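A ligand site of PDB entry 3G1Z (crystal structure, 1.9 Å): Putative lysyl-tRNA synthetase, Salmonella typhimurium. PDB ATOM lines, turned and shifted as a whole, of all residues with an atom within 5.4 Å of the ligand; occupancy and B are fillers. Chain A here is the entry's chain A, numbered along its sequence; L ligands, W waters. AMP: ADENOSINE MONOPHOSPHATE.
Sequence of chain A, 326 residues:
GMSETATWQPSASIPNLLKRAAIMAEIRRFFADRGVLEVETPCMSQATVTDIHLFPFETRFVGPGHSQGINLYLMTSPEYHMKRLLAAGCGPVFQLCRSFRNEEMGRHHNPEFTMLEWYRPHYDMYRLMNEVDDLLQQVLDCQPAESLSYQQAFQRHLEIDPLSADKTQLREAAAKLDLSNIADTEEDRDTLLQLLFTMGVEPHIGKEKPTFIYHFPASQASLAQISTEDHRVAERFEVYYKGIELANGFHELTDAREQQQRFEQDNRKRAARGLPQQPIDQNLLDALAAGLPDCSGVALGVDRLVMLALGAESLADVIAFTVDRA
An oxygen (O2') of the ligand sits close to the guanidinium group of Arg 304, 3.5 Å away. O of Asn 110 sits at hydrogen-bond distance from N6 of the ligand (3.0 Å). An oxygen (O2') of the ligand sits at hydrogen-bond distance from the backbone carbonyl oxygen (O) of Glu 245 (3.1 Å). The backbone NH (N) of Asn 110 is in hydrogen-bond range of a nitrogen (N1) of the ligand (3.2 Å). N of Ala 247 lies within hydrogen-bond range of O3' of the ligand. O1P of the ligand is in salt-bridge range of NH2 of Arg 101. O of Leu 246 sits at hydrogen-bond distance from O2' of the ligand (3.2 Å). OE1 of Glu 103 is in hydrogen-bond range of N6 of the ligand (2.9 Å). An oxygen (O3') of the ligand is in hydrogen-bond range of the side-chain carboxylate of Glu 245, at 2.7 Å.
N of Arg 101 lies within hydrogen-bond range of O of Pro 111. The guanidinium group (NH2) of Arg 304 is in hydrogen-bond range of the backbone carbonyl oxygen (O) of His 108 (2.7 Å). O of Asn 248 lies within hydrogen-bond range of N of Ala 299 (2.8 Å). The backbone carbonyl oxygen (O) of Thr 76 is in hydrogen-bond range of the guanidinium group (NE) of Arg 101, at 3.0 Å. A ring nitrogen (NE2) of His 109 sits at hydrogen-bond distance from the guanidinium group (NH2) of Arg 304. O of Glu 245 lies within hydrogen-bond range of NH1 of Arg 304 (2.9 Å). The backbone carbonyl oxygen (O) of Leu 246 sits at hydrogen-bond distance from the backbone NH (N) of Gly 301 (2.8 Å).
An oxygen (O4') of the ligand sits close to the side-chain sulfur of Met 115 (3.6 Å). Merely in contact with the ligand: His 109 (3.3 Å), Asn 248 (3.4 Å), Phe 113 (3.4 Å), Gly 301 (3.5 Å), His 108 (3.6 Å), Ala 299 (3.6 Å) and Leu 315 (3.7 Å). Hydrophobic or aromatic side chains within 4 Å of the ligand: His 109, Phe 113, Met 115, Ala 299 and Leu 315. Within 4 Å of the ligand: Arg 101, Glu 103, His 108, His 109, Asn 110, Phe 113, Met 115, Glu 245, Leu 246, Ala 247, Asn 248, Ala 299, Gly 301, Arg 304 and Leu 315.
Water W2 lies within hydrogen-bond range of the side-chain carboxylate of Glu 103, a nitrogen (N7) of the ligand and the guanidinium group of Arg 101. Water W4 lies within hydrogen-bond range of N3 of the ligand (3.0 Å), N of Arg 304 (3.2 Å) and N of Asp 303 (3.2 Å).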
ATOM      1  N   LEU A  54      20.487   5.850 -12.855  1.00  0.00           N
ATOM      2  CA  LEU A  54      20.519   5.727 -14.317  1.00  0.00           C
ATOM      3  C   LEU A  54      20.058   4.347 -14.743  1.00  0.00           C
ATOM      4  O   LEU A  54      20.452   3.336 -14.140  1.00  0.00           O
ATOM      5  CB  LEU A  54      21.922   6.054 -14.885  1.00  0.00           C
ATOM      6  CG  LEU A  54      22.349   7.513 -14.925  1.00  0.00           C
ATOM      7  CD1 LEU A  54      23.829   7.659 -15.317  1.00  0.00           C
ATOM      8  CD2 LEU A  54      21.455   8.333 -15.862  1.00  0.00           C
ATOM      9  N   THR A  76      24.565   6.254 -21.814  1.00  0.00           N
ATOM     10  CA  THR A  76      23.751   7.260 -21.145  1.00  0.00           C
ATOM     11  C   THR A  76      24.395   8.608 -21.278  1.00  0.00           C
ATOM     12  O   THR A  76      23.715   9.628 -21.235  1.00  0.00           O
ATOM     13  CB  THR A  76      23.632   6.934 -19.629  1.00  0.00           C
ATOM     14  OG1 THR A  76      24.929   6.985 -19.002  1.00  0.00           O
ATOM     15  CG2 THR A  76      23.001   5.567 -19.404  1.00  0.00           C
ATOM     16  N   SER A  77      25.714   8.589 -21.464  1.00  0.00           N
ATOM     17  CA  SER A  77      26.538   9.768 -21.674  1.00  0.00           C
ATOM     18  C   SER A  77      27.852   9.285 -22.295  1.00  0.00           C
ATOM     19  O   SER A  77      28.318   8.164 -21.998  1.00  0.00           O
ATOM     20  CB  SER A  77      26.767  10.457 -20.319  1.00  0.00           C
ATOM     21  OG  SER A  77      27.963  11.183 -20.300  1.00  0.00           O
ATOM     22  N   ARG A 101      18.797   6.730 -22.479  1.00  0.00           N
ATOM     23  CA  ARG A 101      18.467   6.458 -21.073  1.00  0.00           C
ATOM     24  C   ARG A 101      17.076   5.853 -21.054  1.00  0.00           C
ATOM     25  O   ARG A 101      16.150   6.424 -21.611  1.00  0.00           O
ATOM     26  CB  ARG A 101      18.511   7.745 -20.241  1.00  0.00           C
ATOM     27  CG  ARG A 101      19.933   8.246 -20.063  1.00  0.00           C
ATOM     28  CD  ARG A 101      19.977   9.597 -19.461  1.00  0.00           C
ATOM     29  NE  ARG A 101      21.340  10.126 -19.536  1.00  0.00           N
ATOM     30  CZ  ARG A 101      21.814  11.057 -18.713  1.00  0.00           C
ATOM     31  NH1 ARG A 101      21.041  11.565 -17.770  1.00  0.00           N
ATOM     32  NH2 ARG A 101      23.077  11.500 -18.852  1.00  0.00           N
ATOM     33  N   GLU A 103      14.171   5.659 -19.956  1.00  0.00           N
ATOM     34  CA  GLU A 103      13.275   6.505 -19.173  1.00  0.00           C
ATOM     35  C   GLU A 103      12.031   6.727 -20.022  1.00  0.00           C
ATOM     36  O   GLU A 103      12.142   6.956 -21.237  1.00  0.00           O
ATOM     37  CB  GLU A 103      13.937   7.879 -18.930  1.00  0.00           C
ATOM     38  CG  GLU A 103      15.114   7.860 -17.966  1.00  0.00           C
ATOM     39  CD  GLU A 103      15.777   9.212 -17.815  1.00  0.00           C
ATOM     40  OE1 GLU A 103      15.981   9.924 -18.820  1.00  0.00           O
ATOM     41  OE2 GLU A 103      16.137   9.563 -16.675  1.00  0.00           O
ATOM     42  N   HIS A 108       9.718  16.762 -21.397  1.00  0.00           N
ATOM     43  CA  HIS A 108      11.136  17.156 -21.483  1.00  0.00           C
ATOM     44  C   HIS A 108      12.120  15.965 -21.504  1.00  0.00           C
ATOM     45  O   HIS A 108      13.316  16.159 -21.314  1.00  0.00           O
ATOM     46  CB  HIS A 108      11.548  18.086 -20.331  1.00  0.00           C
ATOM     47  CG  HIS A 108      10.612  19.224 -20.044  1.00  0.00           C
ATOM     48  ND1 HIS A 108      10.005  19.962 -21.034  1.00  0.00           N
ATOM     49  CD2 HIS A 108      10.242  19.786 -18.881  1.00  0.00           C
ATOM     50  CE1 HIS A 108       9.281  20.920 -20.482  1.00  0.00           C
ATOM     51  NE2 HIS A 108       9.402  20.823 -19.172  1.00  0.00           N
ATOM     52  N   HIS A 109      11.626  14.748 -21.700  1.00  0.00           N
ATOM     53  CA  HIS A 109      12.520  13.610 -21.832  1.00  0.00           C
ATOM     54  C   HIS A 109      12.111  12.727 -23.005  1.00  0.00           C
ATOM     55  O   HIS A 109      10.921  12.525 -23.231  1.00  0.00           O
ATOM     56  CB  HIS A 109      12.492  12.723 -20.582  1.00  0.00           C
ATOM     57  CG  HIS A 109      12.897  13.408 -19.306  1.00  0.00           C
ATOM     58  ND1 HIS A 109      12.061  14.280 -18.638  1.00  0.00           N
ATOM     59  CD2 HIS A 109      13.985  13.264 -18.524  1.00  0.00           C
ATOM     60  CE1 HIS A 109      12.640  14.662 -17.520  1.00  0.00           C
ATOM     61  NE2 HIS A 109      13.807  14.062 -17.421  1.00  0.00           N
ATOM     62  N   ASN A 110      13.089  12.212 -23.726  1.00  0.00           N
ATOM     63  CA  ASN A 110      12.895  11.189 -24.745  1.00  0.00           C
ATOM     64  C   ASN A 110      13.975  10.164 -24.425  1.00  0.00           C
ATOM     65  O   ASN A 110      15.036  10.558 -23.920  1.00  0.00           O
ATOM     66  CB  ASN A 110      13.091  11.759 -26.161  1.00  0.00           C
ATOM     67  CG  ASN A 110      12.545  10.842 -27.253  1.00  0.00           C
ATOM     68  OD1 ASN A 110      11.347  10.570 -27.315  1.00  0.00           O
ATOM     69  ND2 ASN A 110      13.452  10.330 -28.120  1.00  0.00           N
ATOM     70  N   PRO A 111      13.702   8.871 -24.643  1.00  0.00           N
ATOM     71  CA  PRO A 111      14.727   7.868 -24.231  1.00  0.00           C
ATOM     72  C   PRO A 111      16.009   7.930 -25.047  1.00  0.00           C
ATOM     73  O   PRO A 111      17.054   7.465 -24.585  1.00  0.00           O
ATOM     74  CB  PRO A 111      14.045   6.521 -24.435  1.00  0.00           C
ATOM     75  CG  PRO A 111      12.893   6.782 -25.346  1.00  0.00           C
ATOM     76  CD  PRO A 111      12.477   8.234 -25.150  1.00  0.00           C
ATOM     77  N   PHE A 113      18.166  11.019 -26.898  1.00  0.00           N
ATOM     78  CA  PHE A 113      18.216  12.477 -27.007  1.00  0.00           C
ATOM     79  C   PHE A 113      19.567  12.972 -27.447  1.00  0.00           C
ATOM     80  O   PHE A 113      20.552  12.255 -27.349  1.00  0.00           O
ATOM     81  CB  PHE A 113      17.811  13.116 -25.669  1.00  0.00           C
ATOM     82  CG  PHE A 113      18.747  12.821 -24.525  1.00  0.00           C
ATOM     83  CD1 PHE A 113      18.669  11.596 -23.829  1.00  0.00           C
ATOM     84  CD2 PHE A 113      19.663  13.771 -24.118  1.00  0.00           C
ATOM     85  CE1 PHE A 113      19.528  11.335 -22.751  1.00  0.00           C
ATOM     86  CE2 PHE A 113      20.537  13.526 -23.042  1.00  0.00           C
ATOM     87  CZ  PHE A 113      20.485  12.330 -22.362  1.00  0.00           C
ATOM     88  N   MET A 115      22.853  14.936 -26.946  1.00  0.00           N
ATOM     89  CA  MET A 115      23.700  15.512 -25.914  1.00  0.00           C
ATOM     90  C   MET A 115      24.833  16.311 -26.540  1.00  0.00           C
ATOM     91  O   MET A 115      25.472  15.849 -27.500  1.00  0.00           O
ATOM     92  CB  MET A 115      24.289  14.435 -24.999  1.00  0.00           C
ATOM     93  CG  MET A 115      25.075  15.043 -23.761  1.00  0.00           C
ATOM     94  SD  MET A 115      23.943  15.511 -22.451  1.00  0.00           S
ATOM     95  CE  MET A 115      23.790  13.887 -21.686  1.00  0.00           C
ATOM     96  N   GLU A 245      15.858  22.393 -16.965  1.00  0.00           N
ATOM     97  CA  GLU A 245      17.223  22.038 -16.645  1.00  0.00           C
ATOM     98  C   GLU A 245      17.979  21.814 -17.960  1.00  0.00           C
ATOM     99  O   GLU A 245      17.652  20.874 -18.707  1.00  0.00           O
ATOM    100  CB  GLU A 245      17.234  20.760 -15.791  1.00  0.00           C
ATOM    101  CG  GLU A 245      18.607  20.274 -15.415  1.00  0.00           C
ATOM    102  CD  GLU A 245      18.634  18.811 -15.089  1.00  0.00           C
ATOM    103  OE1 GLU A 245      17.736  18.366 -14.348  1.00  0.00           O
ATOM    104  OE2 GLU A 245      19.580  18.114 -15.555  1.00  0.00           O
ATOM    105  N   LEU A 246      18.966  22.648 -18.253  1.00  0.00           N
ATOM    106  CA  LEU A 246      19.619  22.588 -19.562  1.00  0.00           C
ATOM    107  C   LEU A 246      20.937  21.823 -19.554  1.00  0.00           C
ATOM    108  O   LEU A 246      21.270  21.119 -20.533  1.00  0.00           O
ATOM    109  CB  LEU A 246      19.857  23.976 -20.112  1.00  0.00           C
ATOM    110  CG  LEU A 246      18.661  24.750 -20.624  1.00  0.00           C
ATOM    111  CD1 LEU A 246      19.139  26.149 -20.934  1.00  0.00           C
ATOM    112  CD2 LEU A 246      18.110  24.080 -21.916  1.00  0.00           C
ATOM    113  N   ALA A 247      21.675  21.913 -18.440  1.00  0.00           N
ATOM    114  CA  ALA A 247      23.047  21.441 -18.397  1.00  0.00           C
ATOM    115  C   ALA A 247      23.583  21.229 -16.981  1.00  0.00           C
ATOM    116  O   ALA A 247      23.173  21.889 -16.033  1.00  0.00           O
ATOM    117  CB  ALA A 247      23.983  22.387 -19.199  1.00  0.00           C
ATOM    118  N   ASN A 248      24.478  20.243 -16.876  1.00  0.00           N
ATOM    119  CA  ASN A 248      25.244  19.963 -15.674  1.00  0.00           C
ATOM    120  C   ASN A 248      26.736  19.951 -16.014  1.00  0.00           C
ATOM    121  O   ASN A 248      27.154  19.310 -16.987  1.00  0.00           O
ATOM    122  CB  ASN A 248      24.820  18.605 -15.095  1.00  0.00           C
ATOM    123  CG  ASN A 248      24.809  18.609 -13.591  1.00  0.00           C
ATOM    124  OD1 ASN A 248      23.821  18.239 -12.964  1.00  0.00           O
ATOM    125  ND2 ASN A 248      25.902  19.090 -13.005  1.00  0.00           N
ATOM    126  N   PHE A 250      30.977  19.928 -14.270  1.00  0.00           N
ATOM    127  CA  PHE A 250      31.724  19.442 -13.116  1.00  0.00           C
ATOM    128  C   PHE A 250      33.204  19.741 -13.271  1.00  0.00           C
ATOM    129  O   PHE A 250      33.711  19.766 -14.385  1.00  0.00           O
ATOM    130  CB  PHE A 250      31.553  17.927 -13.003  1.00  0.00           C
ATOM    131  CG  PHE A 250      30.127  17.454 -13.177  1.00  0.00           C
ATOM    132  CD1 PHE A 250      29.317  17.279 -12.062  1.00  0.00           C
ATOM    133  CD2 PHE A 250      29.613  17.171 -14.450  1.00  0.00           C
ATOM    134  CE1 PHE A 250      27.979  16.800 -12.200  1.00  0.00           C
ATOM    135  CE2 PHE A 250      28.287  16.703 -14.602  1.00  0.00           C
ATOM    136  CZ  PHE A 250      27.484  16.525 -13.463  1.00  0.00           C
ATOM    137  N   ALA A 299      27.687  18.629 -19.642  1.00  0.00           N
ATOM    138  CA  ALA A 299      26.720  17.913 -20.455  1.00  0.00           C
ATOM    139  C   ALA A 299      25.457  18.772 -20.590  1.00  0.00           C
ATOM    140  O   ALA A 299      24.834  19.126 -19.571  1.00  0.00           O
ATOM    141  CB  ALA A 299      26.423  16.571 -19.839  1.00  0.00           C
ATOM    142  N   LEU A 300      25.130  19.124 -21.841  1.00  0.00           N
ATOM    143  CA  LEU A 300      23.978  19.982 -22.149  1.00  0.00           C
ATOM    144  C   LEU A 300      22.953  19.270 -23.049  1.00  0.00           C
ATOM    145  O   LEU A 300      23.318  18.628 -24.068  1.00  0.00           O
ATOM    146  CB  LEU A 300      24.450  21.308 -22.753  1.00  0.00           C
ATOM    147  CG  LEU A 300      23.464  22.429 -23.184  1.00  0.00           C
ATOM    148  CD1 LEU A 300      24.179  23.794 -23.108  1.00  0.00           C
ATOM    149  CD2 LEU A 300      22.965  22.174 -24.626  1.00  0.00           C
ATOM    150  N   GLY A 301      21.689  19.383 -22.654  1.00  0.00           N
ATOM    151  CA  GLY A 301      20.552  18.837 -23.431  1.00  0.00           C
ATOM    152  C   GLY A 301      20.180  19.696 -24.633  1.00  0.00           C
ATOM    153  O   GLY A 301      19.467  20.715 -24.522  1.00  0.00           O
ATOM    154  N   ASP A 303      18.133  19.020 -27.267  1.00  0.00           N
ATOM    155  CA  ASP A 303      16.693  19.051 -27.536  1.00  0.00           C
ATOM    156  C   ASP A 303      15.958  20.115 -26.686  1.00  0.00           C
ATOM    157  O   ASP A 303      15.092  20.824 -27.180  1.00  0.00           O
ATOM    158  CB  ASP A 303      16.088  17.671 -27.387  1.00  0.00           C
ATOM    159  CG  ASP A 303      16.899  16.634 -28.097  1.00  0.00           C
ATOM    160  OD1 ASP A 303      16.983  16.696 -29.336  1.00  0.00           O
ATOM    161  OD2 ASP A 303      17.519  15.794 -27.422  1.00  0.00           O
ATOM    162  N   ARG A 304      16.329  20.231 -25.413  1.00  0.00           N
ATOM    163  CA  ARG A 304      15.803  21.285 -24.558  1.00  0.00           C
ATOM    164  C   ARG A 304      16.289  22.675 -24.997  1.00  0.00           C
ATOM    165  O   ARG A 304      15.522  23.645 -25.005  1.00  0.00           O
ATOM    166  CB  ARG A 304      16.196  21.021 -23.098  1.00  0.00           C
ATOM    167  CG  ARG A 304      15.573  19.735 -22.536  1.00  0.00           C
ATOM    168  CD  ARG A 304      16.018  19.445 -21.088  1.00  0.00           C
ATOM    169  NE  ARG A 304      15.380  18.195 -20.633  1.00  0.00           N
ATOM    170  CZ  ARG A 304      15.495  17.689 -19.408  1.00  0.00           C
ATOM    171  NH1 ARG A 304      16.210  18.312 -18.485  1.00  0.00           N
ATOM    172  NH2 ARG A 304      14.878  16.559 -19.102  1.00  0.00           N
ATOM    173  N   LEU A 315       9.458  18.348 -26.175  1.00  0.00           N
ATOM    174  CA  LEU A 315      10.486  17.798 -27.044  1.00  0.00           C
ATOM    175  C   LEU A 315       9.879  17.273 -28.352  1.00  0.00           C
ATOM    176  O   LEU A 315      10.589  17.107 -29.327  1.00  0.00           O
ATOM    177  CB  LEU A 315      11.270  16.662 -26.303  1.00  0.00           C
ATOM    178  CG  LEU A 315      12.671  16.997 -25.761  1.00  0.00           C
ATOM    179  CD1 LEU A 315      12.834  18.415 -25.238  1.00  0.00           C
ATOM    180  CD2 LEU A 315      13.212  15.996 -24.732  1.00  0.00           C
HETATM  181  P   AMP L   1      23.174  14.457 -17.031  1.00  0.00           P
HETATM  182  O1P AMP L   1      24.154  13.706 -17.913  1.00  0.00           O
HETATM  183  O2P AMP L   1      22.224  13.570 -16.291  1.00  0.00           O
HETATM  184  O3P AMP L   1      23.901  15.510 -16.212  1.00  0.00           O
HETATM  185  O5' AMP L   1      22.206  15.262 -18.035  1.00  0.00           O
HETATM  186  C5' AMP L   1      22.712  16.267 -18.924  1.00  0.00           C
HETATM  187  C4' AMP L   1      21.570  16.994 -19.604  1.00  0.00           C
HETATM  188  O4' AMP L   1      20.924  16.139 -20.582  1.00  0.00           O
HETATM  189  C3' AMP L   1      20.451  17.395 -18.656  1.00  0.00           C
HETATM  190  O3' AMP L   1      20.614  18.683 -18.036  1.00  0.00           O
HETATM  191  C2' AMP L   1      19.245  17.421 -19.556  1.00  0.00           C
HETATM  192  O2' AMP L   1      19.204  18.693 -20.209  1.00  0.00           O
HETATM  193  C1' AMP L   1      19.553  16.414 -20.664  1.00  0.00           C
HETATM  194  N9  AMP L   1      18.818  15.129 -20.522  1.00  0.00           N
HETATM  195  C8  AMP L   1      19.074  14.148 -19.639  1.00  0.00           C
HETATM  196  N7  AMP L   1      18.229  13.104 -19.820  1.00  0.00           N
HETATM  197  C5  AMP L   1      17.405  13.441 -20.836  1.00  0.00           C
HETATM  198  C6  AMP L   1      16.294  12.827 -21.563  1.00  0.00           C
HETATM  199  N6  AMP L   1      15.853  11.604 -21.227  1.00  0.00           N
HETATM  200  N1  AMP L   1      15.746  13.500 -22.588  1.00  0.00           N
HETATM  201  C2  AMP L   1      16.154  14.732 -22.978  1.00  0.00           C
HETATM  202  N3  AMP L   1      17.154  15.365 -22.351  1.00  0.00           N
HETATM  203  C4  AMP L   1      17.811  14.779 -21.303  1.00  0.00           C
HETATM  204  O   HOH W   1      25.696  11.337 -16.340  1.00  0.00           O
HETATM  205  O   HOH W   2      18.100  11.675 -17.189  1.00  0.00           O
HETATM  206  O   HOH W   3      23.162  11.741 -14.289  1.00  0.00           O
HETATM  207  O   HOH W   4      17.621  17.496 -24.468  1.00  0.00           O
